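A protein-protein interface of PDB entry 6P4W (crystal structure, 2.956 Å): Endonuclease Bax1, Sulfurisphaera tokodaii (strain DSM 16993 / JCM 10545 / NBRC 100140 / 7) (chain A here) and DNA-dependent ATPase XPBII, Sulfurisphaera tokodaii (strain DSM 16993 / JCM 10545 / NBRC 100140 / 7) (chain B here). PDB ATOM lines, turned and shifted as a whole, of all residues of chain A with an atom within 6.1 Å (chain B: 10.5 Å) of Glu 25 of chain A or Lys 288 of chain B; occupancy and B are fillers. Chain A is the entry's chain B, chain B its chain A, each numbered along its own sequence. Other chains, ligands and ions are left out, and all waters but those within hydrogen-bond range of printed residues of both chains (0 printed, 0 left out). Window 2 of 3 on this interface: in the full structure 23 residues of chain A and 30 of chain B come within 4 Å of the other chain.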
ATOM      1  N   THR A  23     -16.432  -9.012 -25.376  1.00  0.00           N
ATOM      2  CA  THR A  23     -15.829  -7.987 -26.230  1.00  0.00           C
ATOM      3  C   THR A  23     -14.732  -7.329 -25.428  1.00  0.00           C
ATOM      4  O   THR A  23     -14.436  -7.745 -24.307  1.00  0.00           O
ATOM      5  CB  THR A  23     -16.830  -6.924 -26.686  1.00  0.00           C
ATOM      6  OG1 THR A  23     -17.243  -6.146 -25.556  1.00  0.00           O
ATOM      7  CG2 THR A  23     -18.047  -7.568 -27.311  1.00  0.00           C
ATOM      8  N   ASN A  24     -14.151  -6.265 -25.985  1.00  0.00           N
ATOM      9  CA  ASN A  24     -13.087  -5.574 -25.265  1.00  0.00           C
ATOM     10  C   ASN A  24     -13.597  -4.997 -23.969  1.00  0.00           C
ATOM     11  O   ASN A  24     -12.839  -4.885 -22.998  1.00  0.00           O
ATOM     12  CB  ASN A  24     -12.477  -4.474 -26.113  1.00  0.00           C
ATOM     13  CG  ASN A  24     -11.727  -5.027 -27.269  1.00  0.00           C
ATOM     14  OD1 ASN A  24     -11.124  -6.112 -27.171  1.00  0.00           O
ATOM     15  ND2 ASN A  24     -11.739  -4.293 -28.391  1.00  0.00           N
ATOM     16  N   GLU A  25     -14.891  -4.687 -23.914  1.00  0.00           N
ATOM     17  CA  GLU A  25     -15.475  -4.184 -22.683  1.00  0.00           C
ATOM     18  C   GLU A  25     -15.291  -5.141 -21.513  1.00  0.00           C
ATOM     19  O   GLU A  25     -15.429  -4.719 -20.363  1.00  0.00           O
ATOM     20  CB  GLU A  25     -16.945  -3.877 -22.919  1.00  0.00           C
ATOM     21  CG  GLU A  25     -17.114  -2.790 -23.942  1.00  0.00           C
ATOM     22  CD  GLU A  25     -16.613  -1.455 -23.427  1.00  0.00           C
ATOM     23  OE1 GLU A  25     -16.976  -1.079 -22.287  1.00  0.00           O
ATOM     24  OE2 GLU A  25     -15.826  -0.802 -24.148  1.00  0.00           O
ATOM     25  N   ASP A  26     -14.905  -6.383 -21.763  1.00  0.00           N
ATOM     26  CA  ASP A  26     -14.766  -7.372 -20.712  1.00  0.00           C
ATOM     27  C   ASP A  26     -13.302  -7.615 -20.343  1.00  0.00           C
ATOM     28  O   ASP A  26     -13.006  -8.560 -19.609  1.00  0.00           O
ATOM     29  CB  ASP A  26     -15.483  -8.646 -21.152  1.00  0.00           C
ATOM     30  CG  ASP A  26     -16.990  -8.387 -21.457  1.00  0.00           C
ATOM     31  OD1 ASP A  26     -17.642  -7.643 -20.668  1.00  0.00           O
ATOM     32  OD2 ASP A  26     -17.495  -8.852 -22.521  1.00  0.00           O
ATOM     33  N   LEU A  27     -12.384  -6.765 -20.821  1.00  0.00           N
ATOM     34  CA  LEU A  27     -10.961  -6.968 -20.554  1.00  0.00           C
ATOM     35  C   LEU A  27     -10.634  -6.764 -19.090  1.00  0.00           C
ATOM     36  O   LEU A  27      -9.905  -7.563 -18.493  1.00  0.00           O
ATOM     37  CB  LEU A  27     -10.123  -6.017 -21.394  1.00  0.00           C
ATOM     38  CG  LEU A  27      -9.930  -6.444 -22.833  1.00  0.00           C
ATOM     39  CD1 LEU A  27      -9.368  -5.311 -23.643  1.00  0.00           C
ATOM     40  CD2 LEU A  27      -8.995  -7.602 -22.841  1.00  0.00           C
ATOM     41  N   ASP A  28     -11.143  -5.680 -18.503  1.00  0.00           N
ATOM     42  CA  ASP A  28     -10.980  -5.486 -17.071  1.00  0.00           C
ATOM     43  C   ASP A  28     -11.397  -6.738 -16.316  1.00  0.00           C
ATOM     44  O   ASP A  28     -10.618  -7.287 -15.529  1.00  0.00           O
ATOM     45  CB  ASP A  28     -11.789  -4.283 -16.586  1.00  0.00           C
ATOM     46  CG  ASP A  28     -11.194  -2.954 -17.007  1.00  0.00           C
ATOM     47  OD1 ASP A  28     -10.034  -2.931 -17.487  1.00  0.00           O
ATOM     48  OD2 ASP A  28     -11.877  -1.926 -16.791  1.00  0.00           O
ATOM     49  N   LEU A  29     -12.612  -7.231 -16.571  1.00  0.00           N
ATOM     50  CA  LEU A  29     -13.082  -8.402 -15.843  1.00  0.00           C
ATOM     51  C   LEU A  29     -12.165  -9.583 -16.065  1.00  0.00           C
ATOM     52  O   LEU A  29     -11.841 -10.308 -15.120  1.00  0.00           O
ATOM     53  CB  LEU A  29     -14.491  -8.760 -16.263  1.00  0.00           C
ATOM     54  CG  LEU A  29     -14.990 -10.065 -15.674  1.00  0.00           C
ATOM     55  CD1 LEU A  29     -14.913 -10.095 -14.135  1.00  0.00           C
ATOM     56  CD2 LEU A  29     -16.403 -10.233 -16.145  1.00  0.00           C
ATOM     57  N   ILE A  56     -20.664  -6.682  -9.617  1.00  0.00           N
ATOM     58  CA  ILE A  56     -20.368  -5.613 -10.571  1.00  0.00           C
ATOM     59  C   ILE A  56     -20.712  -6.020 -12.003  1.00  0.00           C
ATOM     60  O   ILE A  56     -21.312  -5.239 -12.747  1.00  0.00           O
ATOM     61  CB  ILE A  56     -18.887  -5.197 -10.439  1.00  0.00           C
ATOM     62  CG1 ILE A  56     -18.571  -4.811  -8.997  1.00  0.00           C
ATOM     63  CG2 ILE A  56     -18.540  -4.072 -11.382  1.00  0.00           C
ATOM     64  CD1 ILE A  56     -17.153  -5.084  -8.583  1.00  0.00           C
ATOM     65  N   TYR A  57     -20.365  -7.250 -12.383  1.00  0.00           N
ATOM     66  CA  TYR A  57     -20.358  -7.727 -13.760  1.00  0.00           C
ATOM     67  C   TYR A  57     -21.361  -8.859 -13.934  1.00  0.00           C
ATOM     68  O   TYR A  57     -21.926  -9.373 -12.956  1.00  0.00           O
ATOM     69  CB  TYR A  57     -18.969  -8.218 -14.163  1.00  0.00           C
ATOM     70  CG  TYR A  57     -17.907  -7.178 -14.080  1.00  0.00           C
ATOM     71  CD1 TYR A  57     -17.961  -6.064 -14.889  1.00  0.00           C
ATOM     72  CD2 TYR A  57     -16.829  -7.332 -13.239  1.00  0.00           C
ATOM     73  CE1 TYR A  57     -16.991  -5.114 -14.841  1.00  0.00           C
ATOM     74  CE2 TYR A  57     -15.839  -6.392 -13.185  1.00  0.00           C
ATOM     75  CZ  TYR A  57     -15.925  -5.282 -13.994  1.00  0.00           C
ATOM     76  OH  TYR A  57     -14.949  -4.320 -13.960  1.00  0.00           O
ATOM     77  N   PHE B 265     -11.279   6.973  -0.162  1.00  0.00           N
ATOM     78  CA  PHE B 265     -11.863   7.002  -1.494  1.00  0.00           C
ATOM     79  C   PHE B 265     -13.221   7.675  -1.476  1.00  0.00           C
ATOM     80  O   PHE B 265     -13.483   8.611  -2.239  1.00  0.00           O
ATOM     81  CB  PHE B 265     -12.023   5.600  -2.058  1.00  0.00           C
ATOM     82  CG  PHE B 265     -12.869   5.560  -3.300  1.00  0.00           C
ATOM     83  CD1 PHE B 265     -12.358   5.984  -4.518  1.00  0.00           C
ATOM     84  CD2 PHE B 265     -14.188   5.126  -3.254  1.00  0.00           C
ATOM     85  CE1 PHE B 265     -13.118   5.953  -5.659  1.00  0.00           C
ATOM     86  CE2 PHE B 265     -14.961   5.105  -4.421  1.00  0.00           C
ATOM     87  CZ  PHE B 265     -14.412   5.510  -5.609  1.00  0.00           C
ATOM     88  N   HIS B 280     -25.541   0.419  -4.343  1.00  0.00           N
ATOM     89  CA  HIS B 280     -25.844   0.295  -5.770  1.00  0.00           C
ATOM     90  C   HIS B 280     -25.043   1.295  -6.594  1.00  0.00           C
ATOM     91  O   HIS B 280     -24.594   0.980  -7.707  1.00  0.00           O
ATOM     92  CB  HIS B 280     -27.352   0.435  -6.011  1.00  0.00           C
ATOM     93  CG  HIS B 280     -28.149  -0.762  -5.566  1.00  0.00           C
ATOM     94  ND1 HIS B 280     -29.524  -0.745  -5.450  1.00  0.00           N
ATOM     95  CD2 HIS B 280     -27.757  -2.006  -5.191  1.00  0.00           C
ATOM     96  CE1 HIS B 280     -29.943  -1.925  -5.023  1.00  0.00           C
ATOM     97  NE2 HIS B 280     -28.890  -2.708  -4.858  1.00  0.00           N
ATOM     98  N   ARG B 281     -24.915   2.528  -6.090  1.00  0.00           N
ATOM     99  CA  ARG B 281     -24.133   3.547  -6.780  1.00  0.00           C
ATOM    100  C   ARG B 281     -22.675   3.127  -6.886  1.00  0.00           C
ATOM    101  O   ARG B 281     -22.047   3.252  -7.945  1.00  0.00           O
ATOM    102  CB  ARG B 281     -24.251   4.879  -6.048  1.00  0.00           C
ATOM    103  CG  ARG B 281     -23.629   5.991  -6.825  1.00  0.00           C
ATOM    104  CD  ARG B 281     -23.768   7.324  -6.185  1.00  0.00           C
ATOM    105  NE  ARG B 281     -23.239   8.332  -7.091  1.00  0.00           N
ATOM    106  CZ  ARG B 281     -23.094   9.607  -6.769  1.00  0.00           C
ATOM    107  NH1 ARG B 281     -22.608  10.481  -7.651  1.00  0.00           N
ATOM    108  NH2 ARG B 281     -23.440   9.999  -5.562  1.00  0.00           N
ATOM    109  N   LEU B 282     -22.113   2.634  -5.782  1.00  0.00           N
ATOM    110  CA  LEU B 282     -20.717   2.227  -5.790  1.00  0.00           C
ATOM    111  C   LEU B 282     -20.506   1.034  -6.732  1.00  0.00           C
ATOM    112  O   LEU B 282     -19.550   1.035  -7.520  1.00  0.00           O
ATOM    113  CB  LEU B 282     -20.274   1.927  -4.362  1.00  0.00           C
ATOM    114  CG  LEU B 282     -18.826   1.456  -4.250  1.00  0.00           C
ATOM    115  CD1 LEU B 282     -17.831   2.484  -4.795  1.00  0.00           C
ATOM    116  CD2 LEU B 282     -18.519   1.074  -2.829  1.00  0.00           C
ATOM    117  N   VAL B 283     -21.403   0.028  -6.699  1.00  0.00           N
ATOM    118  CA  VAL B 283     -21.325  -1.090  -7.648  1.00  0.00           C
ATOM    119  C   VAL B 283     -21.438  -0.592  -9.088  1.00  0.00           C
ATOM    120  O   VAL B 283     -20.725  -1.060  -9.984  1.00  0.00           O
ATOM    121  CB  VAL B 283     -22.394  -2.152  -7.345  1.00  0.00           C
ATOM    122  CG1 VAL B 283     -22.211  -3.356  -8.245  1.00  0.00           C
ATOM    123  CG2 VAL B 283     -22.269  -2.606  -5.954  1.00  0.00           C
ATOM    124  N   LYS B 284     -22.404   0.294  -9.350  1.00  0.00           N
ATOM    125  CA  LYS B 284     -22.537   0.893 -10.676  1.00  0.00           C
ATOM    126  C   LYS B 284     -21.225   1.551 -11.120  1.00  0.00           C
ATOM    127  O   LYS B 284     -20.693   1.236 -12.187  1.00  0.00           O
ATOM    128  CB  LYS B 284     -23.714   1.879 -10.649  1.00  0.00           C
ATOM    129  CG  LYS B 284     -24.007   2.724 -11.890  1.00  0.00           C
ATOM    130  CD  LYS B 284     -23.814   4.219 -11.568  1.00  0.00           C
ATOM    131  CE  LYS B 284     -24.327   5.185 -12.641  1.00  0.00           C
ATOM    132  NZ  LYS B 284     -25.796   5.326 -12.643  1.00  0.00           N
ATOM    133  N   LEU B 285     -20.624   2.384 -10.267  1.00  0.00           N
ATOM    134  CA  LEU B 285     -19.386   3.037 -10.679  1.00  0.00           C
ATOM    135  C   LEU B 285     -18.257   2.025 -10.840  1.00  0.00           C
ATOM    136  O   LEU B 285     -17.316   2.248 -11.613  1.00  0.00           O
ATOM    137  CB  LEU B 285     -19.011   4.114  -9.667  1.00  0.00           C
ATOM    138  CG  LEU B 285     -20.074   5.188  -9.479  1.00  0.00           C
ATOM    139  CD1 LEU B 285     -19.843   5.970  -8.203  1.00  0.00           C
ATOM    140  CD2 LEU B 285     -20.078   6.104 -10.665  1.00  0.00           C
ATOM    141  N   ALA B 286     -18.339   0.899 -10.137  1.00  0.00           N
ATOM    142  CA  ALA B 286     -17.242  -0.054 -10.182  1.00  0.00           C
ATOM    143  C   ALA B 286     -17.144  -0.769 -11.529  1.00  0.00           C
ATOM    144  O   ALA B 286     -16.106  -1.365 -11.831  1.00  0.00           O
ATOM    145  CB  ALA B 286     -17.388  -1.074  -9.044  1.00  0.00           C
ATOM    146  N   ALA B 287     -18.196  -0.722 -12.346  1.00  0.00           N
ATOM    147  CA  ALA B 287     -18.118  -1.368 -13.642  1.00  0.00           C
ATOM    148  C   ALA B 287     -17.079  -0.697 -14.524  1.00  0.00           C
ATOM    149  O   ALA B 287     -16.403  -1.379 -15.299  1.00  0.00           O
ATOM    150  CB  ALA B 287     -19.478  -1.369 -14.318  1.00  0.00           C
ATOM    151  N   LYS B 288     -16.862   0.609 -14.348  1.00  0.00           N
ATOM    152  CA  LYS B 288     -15.973   1.353 -15.227  1.00  0.00           C
ATOM    153  C   LYS B 288     -14.919   2.227 -14.555  1.00  0.00           C
ATOM    154  O   LYS B 288     -14.115   2.819 -15.280  1.00  0.00           O
ATOM    155  CB  LYS B 288     -16.799   2.225 -16.177  1.00  0.00           C
ATOM    156  CG  LYS B 288     -17.741   1.450 -17.056  1.00  0.00           C
ATOM    157  CD  LYS B 288     -17.088   1.224 -18.417  1.00  0.00           C
ATOM    158  CE  LYS B 288     -17.437  -0.168 -18.938  1.00  0.00           C
ATOM    159  NZ  LYS B 288     -16.571  -0.709 -20.008  1.00  0.00           N
ATOM    160  N   ASP B 289     -14.890   2.351 -13.224  1.00  0.00           N
ATOM    161  CA  ASP B 289     -13.810   3.050 -12.521  1.00  0.00           C
ATOM    162  C   ASP B 289     -13.017   2.052 -11.679  1.00  0.00           C
ATOM    163  O   ASP B 289     -13.552   1.479 -10.724  1.00  0.00           O
ATOM    164  CB  ASP B 289     -14.349   4.183 -11.639  1.00  0.00           C
ATOM    165  CG  ASP B 289     -13.226   5.143 -11.123  1.00  0.00           C
ATOM    166  OD1 ASP B 289     -12.037   4.984 -11.515  1.00  0.00           O
ATOM    167  OD2 ASP B 289     -13.544   6.068 -10.326  1.00  0.00           O
ATOM    168  N   LYS B 290     -11.730   1.897 -11.998  1.00  0.00           N
ATOM    169  CA  LYS B 290     -10.888   0.941 -11.283  1.00  0.00           C
ATOM    170  C   LYS B 290     -10.872   1.234  -9.786  1.00  0.00           C
ATOM    171  O   LYS B 290     -11.030   0.322  -8.967  1.00  0.00           O
ATOM    172  CB  LYS B 290      -9.480   0.943 -11.888  1.00  0.00           C
ATOM    173  CG  LYS B 290      -8.437   0.161 -11.139  1.00  0.00           C
ATOM    174  CD  LYS B 290      -8.588  -1.322 -11.299  1.00  0.00           C
ATOM    175  CE  LYS B 290      -7.399  -2.060 -10.679  1.00  0.00           C
ATOM    176  NZ  LYS B 290      -7.603  -3.547 -10.670  1.00  0.00           N
ATOM    177  N   GLU B 291     -10.706   2.509  -9.405  1.00  0.00           N
ATOM    178  CA  GLU B 291     -10.581   2.858  -7.988  1.00  0.00           C
ATOM    179  C   GLU B 291     -11.872   2.564  -7.221  1.00  0.00           C
ATOM    180  O   GLU B 291     -11.825   2.188  -6.042  1.00  0.00           O
ATOM    181  CB  GLU B 291     -10.223   4.336  -7.837  1.00  0.00           C
ATOM    182  CG  GLU B 291      -8.891   4.738  -8.446  1.00  0.00           C
ATOM    183  CD  GLU B 291      -8.750   6.255  -8.659  1.00  0.00           C
ATOM    184  OE1 GLU B 291      -9.775   6.969  -8.629  1.00  0.00           O
ATOM    185  OE2 GLU B 291      -7.609   6.732  -8.856  1.00  0.00           O
ATOM    186  N   ALA B 292     -13.039   2.730  -7.860  1.00  0.00           N
ATOM    187  CA  ALA B 292     -14.280   2.327  -7.201  1.00  0.00           C
ATOM    188  C   ALA B 292     -14.298   0.824  -6.961  1.00  0.00           C
ATOM    189  O   ALA B 292     -14.676   0.378  -5.875  1.00  0.00           O
ATOM    190  CB  ALA B 292     -15.500   2.768  -8.006  1.00  0.00           C
ATOM    191  N   ARG B 293     -13.888   0.030  -7.959  1.00  0.00           N
ATOM    192  CA  ARG B 293     -13.764  -1.412  -7.774  1.00  0.00           C
ATOM    193  C   ARG B 293     -12.906  -1.758  -6.574  1.00  0.00           C
ATOM    194  O   ARG B 293     -13.280  -2.607  -5.758  1.00  0.00           O
ATOM    195  CB  ARG B 293     -13.182  -2.067  -9.013  1.00  0.00           C
ATOM    196  CG  ARG B 293     -14.150  -2.870  -9.793  1.00  0.00           C
ATOM    197  CD  ARG B 293     -13.439  -3.913 -10.585  1.00  0.00           C
ATOM    198  NE  ARG B 293     -12.315  -3.457 -11.422  1.00  0.00           N
ATOM    199  CZ  ARG B 293     -12.383  -2.600 -12.441  1.00  0.00           C
ATOM    200  NH1 ARG B 293     -13.516  -2.018 -12.766  1.00  0.00           N
ATOM    201  NH2 ARG B 293     -11.292  -2.313 -13.135  1.00  0.00           N
ATOM    202  N   GLU B 294     -11.714  -1.173  -6.490  1.00  0.00           N
ATOM    203  CA  GLU B 294     -10.835  -1.525  -5.377  1.00  0.00           C
ATOM    204  C   GLU B 294     -11.451  -1.128  -4.040  1.00  0.00           C
ATOM    205  O   GLU B 294     -11.231  -1.811  -3.024  1.00  0.00           O
ATOM    206  CB  GLU B 294      -9.442  -0.904  -5.559  1.00  0.00           C
ATOM    207  CG  GLU B 294      -8.840  -1.192  -6.911  1.00  0.00           C
ATOM    208  CD  GLU B 294      -7.542  -0.454  -7.159  1.00  0.00           C
ATOM    209  OE1 GLU B 294      -6.616  -1.078  -7.722  1.00  0.00           O
ATOM    210  OE2 GLU B 294      -7.440   0.737  -6.790  1.00  0.00           O
ATOM    211  N   LEU B 296     -14.743  -1.143  -3.433  1.00  0.00           N
ATOM    212  CA  LEU B 296     -15.724  -2.162  -3.159  1.00  0.00           C
ATOM    213  C   LEU B 296     -15.021  -3.443  -2.758  1.00  0.00           C
ATOM    214  O   LEU B 296     -15.531  -4.201  -1.923  1.00  0.00           O
ATOM    215  CB  LEU B 296     -16.617  -2.333  -4.386  1.00  0.00           C
ATOM    216  CG  LEU B 296     -17.885  -3.170  -4.256  1.00  0.00           C
ATOM    217  CD1 LEU B 296     -18.741  -2.763  -3.042  1.00  0.00           C
ATOM    218  CD2 LEU B 296     -18.674  -3.068  -5.548  1.00  0.00           C
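The guanidinium group of Arg 293 of chain B lies within hydrogen-bond range of the side-chain hydroxyl of Tyr 57 of chain A (3.0 Å). NZ of Lys 288 of chain B sits close to OE1 of Glu 25 of chain A (2.3 Å). The guanidinium group of Arg 293 of chain B lies within salt-bridge range of the side-chain carboxylate of Asp 28 of chain A, 3.7 Å away.
The guanidinium group (NH1) of Arg 293 of chain B lies within hydrogen-bond range of the backbone carbonyl oxygen (O) of Ala 286 of chain B, 2.8 Å away. OG1 of Thr 23 of chain A sits close to N of Glu 25 of chain A (3.2 Å).
Ile 56 of chain A touches Val 283 of chain B (CA to CG1, 3.7 Å). Ile 56 of chain A touches Ala 286 of chain B (CG2 to C, 3.6 Å). Ile 56 of chain A touches Ala 287 of chain B (CG2 to N, 3.5 Å). Arg 293 of chain B touches Ile 56 of chain A (CG to CD1, 3.9 Å). Leu 296 of chain B touches Ile 56 of chain A. O of Ala 286 of chain B touches OH of Tyr 57 of chain A, 3.8 Å away. OH of Tyr 57 of chain A touches O of Ala 287 of chain B, 3.5 Å away.
Glu 25 of chain A touches one residue of chain B. Lys 288 of chain B touches just one residue of chain A: Glu 25 (2.3 Å). No residue of chain B comes within 4 Å of Thr 23 of chain A. No residue of chain B comes within 4 Å of Asn 24 of chain A. No residue of chain B comes within 4 Å of Asp 26 of chain A. Printed residues of chain B within 4 Å of Ile 56 of chain A: Val 283 (3.7 Å), Ala 286 (3.6 Å), Ala 287 (3.5 Å), Arg 293 (3.9 Å) and Leu 296 (3.9 Å). Of the printed residues of chain A, Ala 287 of chain B touches Ile 56 and Tyr 57. Of the printed residues of chain A, Val 283 of chain B touches Ile 56 (3.7 Å). Of the printed residues of chain B, Tyr 57 of chain A touches Ala 286, Ala 287 and Arg 293. Leu 282 of chain B touches none of the printed residues of chain A. Leu 285 of chain B touches none of the printed residues of chain A. The nearest residue of chain A that does not touch Lys 288 of chain B is Tyr 57 of chain A (5.3 Å).
Hydrophobic or aromatic side chains of chain A within 4 Å of the printed part of chain B: Ile 56 and Tyr 57. Of the 17 printed residues of chain B, 6 touch a printed residue of chain A. Hydrophobic or aromatic side chains of chain B that line the printed part of chain A: Val 283, Ala 286 and Leu 296. Among the printed residues, Asp or Glu carboxylates within 4 Å of a Lys or Arg side-chain nitrogen of the other chain: Glu 25 of chain A with Lys 288 of chain B (2.3 Å) and Asp 28 of chain A with Arg 293 of chain B (3.7 Å).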
